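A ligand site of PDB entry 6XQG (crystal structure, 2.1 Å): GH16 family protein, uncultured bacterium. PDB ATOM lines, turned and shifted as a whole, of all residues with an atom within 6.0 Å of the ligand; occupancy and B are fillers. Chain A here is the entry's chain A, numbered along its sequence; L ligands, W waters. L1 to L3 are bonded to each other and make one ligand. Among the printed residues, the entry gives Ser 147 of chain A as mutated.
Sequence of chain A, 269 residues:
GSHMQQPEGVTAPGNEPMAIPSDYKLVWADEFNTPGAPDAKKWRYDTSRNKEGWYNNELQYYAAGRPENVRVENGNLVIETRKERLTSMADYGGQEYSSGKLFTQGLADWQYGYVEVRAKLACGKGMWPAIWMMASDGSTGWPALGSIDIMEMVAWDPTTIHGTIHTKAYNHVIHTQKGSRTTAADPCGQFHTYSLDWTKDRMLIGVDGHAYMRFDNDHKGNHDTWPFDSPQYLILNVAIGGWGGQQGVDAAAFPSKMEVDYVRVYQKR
Water W6 lies within hydrogen-bond range of O6 of LIG L1 (2.6 Å), O of Trp 128 (3.1 Å) and ND2 of Asn 237 (3.3 Å).
Water W4 lies within hydrogen-bond range of the side-chain carboxylate of Glu 58 (2.7 Å) and an oxygen (O4) of LIG L1 (2.8 Å).
Water W3 lies within hydrogen-bond range of an oxygen (O2) of LG2 L2 (2.8 Å) and the side-chain amide oxygen (OD1) of Asn 56 (3.1 Å).
Water W8 bridges an oxygen (O2) of LG3 L3 (3.0 Å) and the backbone NH of Trp 142 (3.1 Å).
ND2 of Asn 56 sits at hydrogen-bond distance from OE2 of Glu 58 (2.9 Å).
OE2 of Glu 152 is in hydrogen-bond range of NE1 of Trp 128 (2.7 Å).
The backbone NH of His 166 lies within hydrogen-bond range of the backbone carbonyl oxygen of Ser 147, 2.9 Å away.
The backbone NH (N) of Ala 130 sits at hydrogen-bond distance from the backbone carbonyl oxygen (O) of Asn 237, 2.9 Å away.
N of Trp 128 lies within hydrogen-bond range of O of Ala 239 (2.8 Å).
NE1 of Trp 132 sits at hydrogen-bond distance from OD1 of Asn 237.
Tyr 55 touches the ligand.
CB of Ala 130 touches O6 of LIG L1, at 3.7 Å.
Trp 132 touches the ligand.
SD of Met 134 touches C5 of LG2 L2, 3.8 Å away.
CZ2 of Trp 142 touches O2 of LIG L1, at 3.0 Å.
NE2 of His 166 touches O2 of LIG L1, at 3.5 Å.
Of the 19 residues printed, 10 come within 4 Å of the ligand.
The indole nitrogen (NE1) of Trp 128 lies close to an oxygen (O6) of LIG L1.
OD1 of Asn 56 sits at hydrogen-bond distance from O1 of LG2 L2.
O6 of LIG L1 sits at hydrogen-bond distance from OE2 of Glu 152 (2.8 Å).
OD1 of Asp 149 is in hydrogen-bond range of O1 of LIG L1 (2.7 Å).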
ATOM      1  N   TRP A  54     -10.690  20.100 -13.872  1.00  0.00           N
ATOM      2  CA  TRP A  54     -11.851  20.576 -13.101  1.00  0.00           C
ATOM      3  C   TRP A  54     -11.641  22.017 -12.576  1.00  0.00           C
ATOM      4  O   TRP A  54     -10.579  22.639 -12.790  1.00  0.00           O
ATOM      5  CB  TRP A  54     -12.190  19.550 -12.003  1.00  0.00           C
ATOM      6  CG  TRP A  54     -12.795  18.319 -12.587  1.00  0.00           C
ATOM      7  CD1 TRP A  54     -12.131  17.198 -13.021  1.00  0.00           C
ATOM      8  CD2 TRP A  54     -14.182  18.105 -12.862  1.00  0.00           C
ATOM      9  NE1 TRP A  54     -13.010  16.309 -13.544  1.00  0.00           N
ATOM     10  CE2 TRP A  54     -14.279  16.827 -13.471  1.00  0.00           C
ATOM     11  CE3 TRP A  54     -15.342  18.834 -12.635  1.00  0.00           C
ATOM     12  CZ2 TRP A  54     -15.501  16.299 -13.884  1.00  0.00           C
ATOM     13  CZ3 TRP A  54     -16.551  18.307 -13.051  1.00  0.00           C
ATOM     14  CH2 TRP A  54     -16.636  17.048 -13.637  1.00  0.00           C
ATOM     15  N   TYR A  55     -12.691  22.605 -12.032  1.00  0.00           N
ATOM     16  CA  TYR A  55     -12.698  24.039 -11.650  1.00  0.00           C
ATOM     17  C   TYR A  55     -11.861  24.180 -10.370  1.00  0.00           C
ATOM     18  O   TYR A  55     -11.465  23.171  -9.810  1.00  0.00           O
ATOM     19  CB  TYR A  55     -14.152  24.499 -11.542  1.00  0.00           C
ATOM     20  CG  TYR A  55     -14.947  24.329 -12.812  1.00  0.00           C
ATOM     21  CD1 TYR A  55     -14.732  25.140 -13.917  1.00  0.00           C
ATOM     22  CD2 TYR A  55     -15.917  23.346 -12.902  1.00  0.00           C
ATOM     23  CE1 TYR A  55     -15.487  25.001 -15.074  1.00  0.00           C
ATOM     24  CE2 TYR A  55     -16.650  23.172 -14.068  1.00  0.00           C
ATOM     25  CZ  TYR A  55     -16.447  23.997 -15.157  1.00  0.00           C
ATOM     26  OH  TYR A  55     -17.199  23.810 -16.289  1.00  0.00           O
ATOM     27  N   ASN A  56     -11.614  25.404  -9.906  1.00  0.00           N
ATOM     28  CA  ASN A  56     -11.012  25.647  -8.569  1.00  0.00           C
ATOM     29  C   ASN A  56      -9.530  25.192  -8.563  1.00  0.00           C
ATOM     30  O   ASN A  56      -8.996  24.838  -7.507  1.00  0.00           O
ATOM     31  CB  ASN A  56     -11.865  24.986  -7.461  1.00  0.00           C
ATOM     32  CG  ASN A  56     -13.337  25.373  -7.481  1.00  0.00           C
ATOM     33  OD1 ASN A  56     -13.667  26.550  -7.629  1.00  0.00           O
ATOM     34  ND2 ASN A  56     -14.224  24.411  -7.315  1.00  0.00           N
ATOM     35  N   GLU A  58      -8.528  22.421  -9.286  1.00  0.00           N
ATOM     36  CA  GLU A  58      -8.603  21.038  -8.709  1.00  0.00           C
ATOM     37  C   GLU A  58      -7.614  20.135  -9.448  1.00  0.00           C
ATOM     38  O   GLU A  58      -7.319  20.409 -10.603  1.00  0.00           O
ATOM     39  CB  GLU A  58     -10.042  20.549  -8.746  1.00  0.00           C
ATOM     40  CG  GLU A  58     -10.850  21.167  -7.625  1.00  0.00           C
ATOM     41  CD  GLU A  58     -12.347  20.980  -7.774  1.00  0.00           C
ATOM     42  OE1 GLU A  58     -12.772  20.042  -8.482  1.00  0.00           O
ATOM     43  OE2 GLU A  58     -13.097  21.714  -7.153  1.00  0.00           O
ATOM     44  N   LYS A 101     -16.914  11.366  -8.250  1.00  0.00           N
ATOM     45  CA  LYS A 101     -18.015  12.360  -8.203  1.00  0.00           C
ATOM     46  C   LYS A 101     -19.286  11.734  -8.756  1.00  0.00           C
ATOM     47  O   LYS A 101     -19.320  11.420  -9.945  1.00  0.00           O
ATOM     48  CB  LYS A 101     -17.694  13.616  -9.010  1.00  0.00           C
ATOM     49  CG  LYS A 101     -18.826  14.641  -8.964  1.00  0.00           C
ATOM     50  CD  LYS A 101     -18.475  15.966  -9.593  1.00  0.00           C
ATOM     51  CE  LYS A 101     -19.468  17.085  -9.370  1.00  0.00           C
ATOM     52  NZ  LYS A 101     -19.345  18.116 -10.454  1.00  0.00           N
ATOM     53  N   TRP A 128     -10.676  17.350  -0.237  1.00  0.00           N
ATOM     54  CA  TRP A 128     -11.809  18.306  -0.186  1.00  0.00           C
ATOM     55  C   TRP A 128     -13.097  17.531  -0.439  1.00  0.00           C
ATOM     56  O   TRP A 128     -13.727  17.616  -1.521  1.00  0.00           O
ATOM     57  CB  TRP A 128     -11.507  19.488  -1.121  1.00  0.00           C
ATOM     58  CG  TRP A 128     -12.550  20.569  -1.200  1.00  0.00           C
ATOM     59  CD1 TRP A 128     -13.606  20.790  -0.349  1.00  0.00           C
ATOM     60  CD2 TRP A 128     -12.611  21.606  -2.202  1.00  0.00           C
ATOM     61  NE1 TRP A 128     -14.288  21.929  -0.723  1.00  0.00           N
ATOM     62  CE2 TRP A 128     -13.708  22.433  -1.867  1.00  0.00           C
ATOM     63  CE3 TRP A 128     -11.812  21.939  -3.304  1.00  0.00           C
ATOM     64  CZ2 TRP A 128     -14.050  23.535  -2.653  1.00  0.00           C
ATOM     65  CZ3 TRP A 128     -12.141  23.036  -4.071  1.00  0.00           C
ATOM     66  CH2 TRP A 128     -13.253  23.822  -3.748  1.00  0.00           C
ATOM     67  N   PRO A 129     -13.541  16.760   0.579  1.00  0.00           N
ATOM     68  CA  PRO A 129     -14.802  16.056   0.518  1.00  0.00           C
ATOM     69  C   PRO A 129     -15.964  17.063   0.528  1.00  0.00           C
ATOM     70  O   PRO A 129     -15.850  18.044   1.235  1.00  0.00           O
ATOM     71  CB  PRO A 129     -14.790  15.192   1.788  1.00  0.00           C
ATOM     72  CG  PRO A 129     -14.014  16.003   2.760  1.00  0.00           C
ATOM     73  CD  PRO A 129     -12.896  16.563   1.898  1.00  0.00           C
ATOM     74  N   ALA A 130     -17.045  16.765  -0.191  1.00  0.00           N
ATOM     75  CA  ALA A 130     -18.213  17.656  -0.275  1.00  0.00           C
ATOM     76  C   ALA A 130     -19.503  16.845  -0.424  1.00  0.00           C
ATOM     77  O   ALA A 130     -19.475  15.720  -0.984  1.00  0.00           O
ATOM     78  CB  ALA A 130     -18.050  18.584  -1.464  1.00  0.00           C
ATOM     79  N   TRP A 132     -23.316  18.398  -1.562  1.00  0.00           N
ATOM     80  CA  TRP A 132     -23.800  19.721  -2.028  1.00  0.00           C
ATOM     81  C   TRP A 132     -24.798  19.497  -3.155  1.00  0.00           C
ATOM     82  O   TRP A 132     -25.059  18.306  -3.547  1.00  0.00           O
ATOM     83  CB  TRP A 132     -22.622  20.629  -2.362  1.00  0.00           C
ATOM     84  CG  TRP A 132     -21.723  20.179  -3.477  1.00  0.00           C
ATOM     85  CD1 TRP A 132     -20.965  19.062  -3.497  1.00  0.00           C
ATOM     86  CD2 TRP A 132     -21.453  20.864  -4.723  1.00  0.00           C
ATOM     87  NE1 TRP A 132     -20.302  18.955  -4.698  1.00  0.00           N
ATOM     88  CE2 TRP A 132     -20.531  20.066  -5.435  1.00  0.00           C
ATOM     89  CE3 TRP A 132     -21.916  22.039  -5.328  1.00  0.00           C
ATOM     90  CZ2 TRP A 132     -20.058  20.414  -6.705  1.00  0.00           C
ATOM     91  CZ3 TRP A 132     -21.452  22.392  -6.571  1.00  0.00           C
ATOM     92  CH2 TRP A 132     -20.522  21.591  -7.250  1.00  0.00           C
ATOM     93  N   MET A 134     -26.962  21.585  -6.632  1.00  0.00           N
ATOM     94  CA  MET A 134     -27.079  22.649  -7.641  1.00  0.00           C
ATOM     95  C   MET A 134     -28.473  22.508  -8.248  1.00  0.00           C
ATOM     96  O   MET A 134     -28.998  21.380  -8.237  1.00  0.00           O
ATOM     97  CB  MET A 134     -25.994  22.565  -8.719  1.00  0.00           C
ATOM     98  CG  MET A 134     -24.634  23.175  -8.316  1.00  0.00           C
ATOM     99  SD  MET A 134     -23.519  23.461  -9.754  1.00  0.00           S
ATOM    100  CE  MET A 134     -23.214  21.731 -10.114  1.00  0.00           C
ATOM    101  N   GLY A 141     -26.915  30.364 -15.217  1.00  0.00           N
ATOM    102  CA  GLY A 141     -25.468  30.152 -15.011  1.00  0.00           C
ATOM    103  C   GLY A 141     -24.998  30.133 -13.547  1.00  0.00           C
ATOM    104  O   GLY A 141     -25.848  30.081 -12.595  1.00  0.00           O
ATOM    105  N   TRP A 142     -23.670  30.144 -13.367  1.00  0.00           N
ATOM    106  CA  TRP A 142     -22.989  30.143 -12.050  1.00  0.00           C
ATOM    107  C   TRP A 142     -22.537  31.561 -11.738  1.00  0.00           C
ATOM    108  O   TRP A 142     -21.937  32.196 -12.605  1.00  0.00           O
ATOM    109  CB  TRP A 142     -21.791  29.167 -11.994  1.00  0.00           C
ATOM    110  CG  TRP A 142     -21.111  29.159 -10.653  1.00  0.00           C
ATOM    111  CD1 TRP A 142     -20.091  29.960 -10.235  1.00  0.00           C
ATOM    112  CD2 TRP A 142     -21.436  28.308  -9.530  1.00  0.00           C
ATOM    113  NE1 TRP A 142     -19.779  29.667  -8.936  1.00  0.00           N
ATOM    114  CE2 TRP A 142     -20.585  28.649  -8.486  1.00  0.00           C
ATOM    115  CE3 TRP A 142     -22.367  27.290  -9.323  1.00  0.00           C
ATOM    116  CZ2 TRP A 142     -20.620  27.997  -7.254  1.00  0.00           C
ATOM    117  CZ3 TRP A 142     -22.425  26.665  -8.089  1.00  0.00           C
ATOM    118  CH2 TRP A 142     -21.552  27.003  -7.074  1.00  0.00           C
ATOM    119  N   SER A 147     -26.875  27.343  -5.336  1.00  0.00           N
ATOM    120  CA  SER A 147     -26.082  26.157  -4.941  1.00  0.00           C
ATOM    121  C   SER A 147     -26.100  26.034  -3.417  1.00  0.00           C
ATOM    122  O   SER A 147     -26.042  27.096  -2.735  1.00  0.00           O
ATOM    123  CB  SER A 147     -24.697  26.304  -5.438  1.00  0.00           C
ATOM    124  OG  SER A 147     -24.158  25.031  -5.628  1.00  0.00           O
ATOM    125  N   ILE A 148     -26.178  24.824  -2.888  1.00  0.00           N
ATOM    126  CA  ILE A 148     -26.236  24.576  -1.414  1.00  0.00           C
ATOM    127  C   ILE A 148     -25.127  23.589  -1.067  1.00  0.00           C
ATOM    128  O   ILE A 148     -25.161  22.440  -1.590  1.00  0.00           O
ATOM    129  CB  ILE A 148     -27.613  23.996  -1.045  1.00  0.00           C
ATOM    130  CG1 ILE A 148     -28.769  24.796  -1.643  1.00  0.00           C
ATOM    131  CG2 ILE A 148     -27.750  23.860   0.466  1.00  0.00           C
ATOM    132  CD1 ILE A 148     -30.006  23.963  -1.944  1.00  0.00           C
ATOM    133  N   ASP A 149     -24.188  24.007  -0.235  1.00  0.00           N
ATOM    134  CA  ASP A 149     -23.164  23.098   0.326  1.00  0.00           C
ATOM    135  C   ASP A 149     -23.623  22.684   1.718  1.00  0.00           C
ATOM    136  O   ASP A 149     -23.448  23.490   2.650  1.00  0.00           O
ATOM    137  CB  ASP A 149     -21.772  23.730   0.389  1.00  0.00           C
ATOM    138  CG  ASP A 149     -21.132  23.787  -0.999  1.00  0.00           C
ATOM    139  OD1 ASP A 149     -21.586  24.628  -1.819  1.00  0.00           O
ATOM    140  OD2 ASP A 149     -20.182  22.972  -1.248  1.00  0.00           O
ATOM    141  N   GLU A 152     -18.980  20.978   3.601  1.00  0.00           N
ATOM    142  CA  GLU A 152     -17.652  21.070   2.975  1.00  0.00           C
ATOM    143  C   GLU A 152     -16.602  20.984   4.071  1.00  0.00           C
ATOM    144  O   GLU A 152     -16.761  21.627   5.107  1.00  0.00           O
ATOM    145  CB  GLU A 152     -17.570  22.366   2.190  1.00  0.00           C
ATOM    146  CG  GLU A 152     -17.969  22.248   0.736  1.00  0.00           C
ATOM    147  CD  GLU A 152     -17.558  23.508   0.002  1.00  0.00           C
ATOM    148  OE1 GLU A 152     -18.185  24.599   0.279  1.00  0.00           O
ATOM    149  OE2 GLU A 152     -16.553  23.442  -0.744  1.00  0.00           O
ATOM    150  N   HIS A 166     -24.795  29.644  -2.400  1.00  0.00           N
ATOM    151  CA  HIS A 166     -24.221  30.468  -3.499  1.00  0.00           C
ATOM    152  C   HIS A 166     -25.384  30.988  -4.327  1.00  0.00           C
ATOM    153  O   HIS A 166     -26.231  30.134  -4.710  1.00  0.00           O
ATOM    154  CB  HIS A 166     -23.283  29.618  -4.370  1.00  0.00           C
ATOM    155  CG  HIS A 166     -22.053  29.165  -3.631  1.00  0.00           C
ATOM    156  ND1 HIS A 166     -20.931  29.971  -3.512  1.00  0.00           N
ATOM    157  CD2 HIS A 166     -21.802  28.017  -2.963  1.00  0.00           C
ATOM    158  CE1 HIS A 166     -20.016  29.325  -2.808  1.00  0.00           C
ATOM    159  NE2 HIS A 166     -20.525  28.126  -2.456  1.00  0.00           N
ATOM    160  N   ASN A 237     -18.639  13.981  -3.645  1.00  0.00           N
ATOM    161  CA  ASN A 237     -17.320  13.967  -4.315  1.00  0.00           C
ATOM    162  C   ASN A 237     -16.243  14.243  -3.292  1.00  0.00           C
ATOM    163  O   ASN A 237     -16.541  14.829  -2.244  1.00  0.00           O
ATOM    164  CB  ASN A 237     -17.328  14.965  -5.465  1.00  0.00           C
ATOM    165  CG  ASN A 237     -17.381  16.393  -4.976  1.00  0.00           C
ATOM    166  OD1 ASN A 237     -18.440  16.811  -4.494  1.00  0.00           O
ATOM    167  ND2 ASN A 237     -16.248  17.111  -5.019  1.00  0.00           N
ATOM    168  N   ALA A 239     -12.851  16.240  -4.055  1.00  0.00           N
ATOM    169  CA  ALA A 239     -11.848  17.043  -4.780  1.00  0.00           C
ATOM    170  C   ALA A 239     -10.559  16.956  -3.985  1.00  0.00           C
ATOM    171  O   ALA A 239     -10.563  16.429  -2.827  1.00  0.00           O
ATOM    172  CB  ALA A 239     -12.318  18.476  -5.006  1.00  0.00           C
HETATM  173  C1  LIG L   1     -18.887  25.104  -3.526  1.00  0.00           C
HETATM  174  C2  LIG L   1     -18.063  25.715  -4.679  1.00  0.00           C
HETATM  175  C3  LIG L   1     -17.808  24.684  -5.802  1.00  0.00           C
HETATM  176  C4  LIG L   1     -17.200  23.413  -5.201  1.00  0.00           C
HETATM  177  C5  LIG L   1     -18.228  22.859  -4.206  1.00  0.00           C
HETATM  178  C6  LIG L   1     -17.833  21.476  -3.765  1.00  0.00           C
HETATM  179  O1  LIG L   1     -20.192  24.928  -4.104  1.00  0.00           O
HETATM  180  O2  LIG L   1     -18.791  26.808  -5.255  1.00  0.00           O
HETATM  181  O3  LIG L   1     -17.018  25.217  -6.937  1.00  0.00           O
HETATM  182  O4  LIG L   1     -16.949  22.456  -6.256  1.00  0.00           O
HETATM  183  O5  LIG L   1     -18.429  23.792  -3.100  1.00  0.00           O
HETATM  184  O6  LIG L   1     -16.714  21.688  -2.921  1.00  0.00           O
HETATM  185  C1  LG2 L   2     -16.579  26.577  -9.044  1.00  0.00           C
HETATM  186  C2  LG2 L   2     -17.370  27.093 -10.265  1.00  0.00           C
HETATM  187  C3  LG2 L   2     -18.258  25.970 -10.838  1.00  0.00           C
HETATM  188  C4  LG2 L   2     -19.070  25.288  -9.743  1.00  0.00           C
HETATM  189  C5  LG2 L   2     -19.867  24.104 -10.321  1.00  0.00           C
HETATM  190  C6  LG2 L   2     -17.447  25.906  -7.999  1.00  0.00           C
HETATM  191  O1  LG2 L   2     -15.933  27.678  -8.453  1.00  0.00           O
HETATM  192  O2  LG2 L   2     -16.471  27.633 -11.223  1.00  0.00           O
HETATM  193  O3  LG2 L   2     -19.186  26.521 -11.800  1.00  0.00           O
HETATM  194  O4  LG2 L   2     -18.300  24.907  -8.599  1.00  0.00           O
HETATM  195  O5  LG2 L   2     -19.080  23.115 -10.928  1.00  0.00           O
HETATM  196  C1  LG3 L   3     -19.855  26.679 -14.092  1.00  0.00           C
HETATM  197  C2  LG3 L   3     -19.409  26.997 -15.507  1.00  0.00           C
HETATM  198  C3  LG3 L   3     -18.667  28.327 -15.493  1.00  0.00           C
HETATM  199  C4  LG3 L   3     -17.593  28.314 -14.425  1.00  0.00           C
HETATM  200  C5  LG3 L   3     -16.988  29.730 -14.320  1.00  0.00           C
HETATM  201  C6  LG3 L   3     -18.723  26.636 -13.090  1.00  0.00           C
HETATM  202  O1  LG3 L   3     -20.492  25.465 -14.026  1.00  0.00           O
HETATM  203  O2  LG3 L   3     -20.575  27.165 -16.309  1.00  0.00           O
HETATM  204  O3  LG3 L   3     -18.014  28.609 -16.761  1.00  0.00           O
HETATM  205  O4  LG3 L   3     -18.126  27.918 -13.151  1.00  0.00           O
HETATM  206  O5  LG3 L   3     -15.775  29.545 -13.598  1.00  0.00           O
HETATM  207  O   HOH W   1     -20.181  21.660 -12.797  1.00  0.00           O
HETATM  208  O   HOH W   2     -22.989  25.489 -12.949  1.00  0.00           O
HETATM  209  O   HOH W   3     -13.805  27.933 -10.384  1.00  0.00           O
HETATM  210  O   HOH W   4     -15.022  20.524  -5.754  1.00  0.00           O
HETATM  211  O   HOH W   5     -16.950  28.754  -5.871  1.00  0.00           O
HETATM  212  O   HOH W   6     -15.172  19.663  -3.270  1.00  0.00           O
HETATM  213  O   HOH W   7     -17.150  22.423  -9.139  1.00  0.00           O
HETATM  214  O   HOH W   8     -22.096  29.732 -15.947  1.00  0.00           O
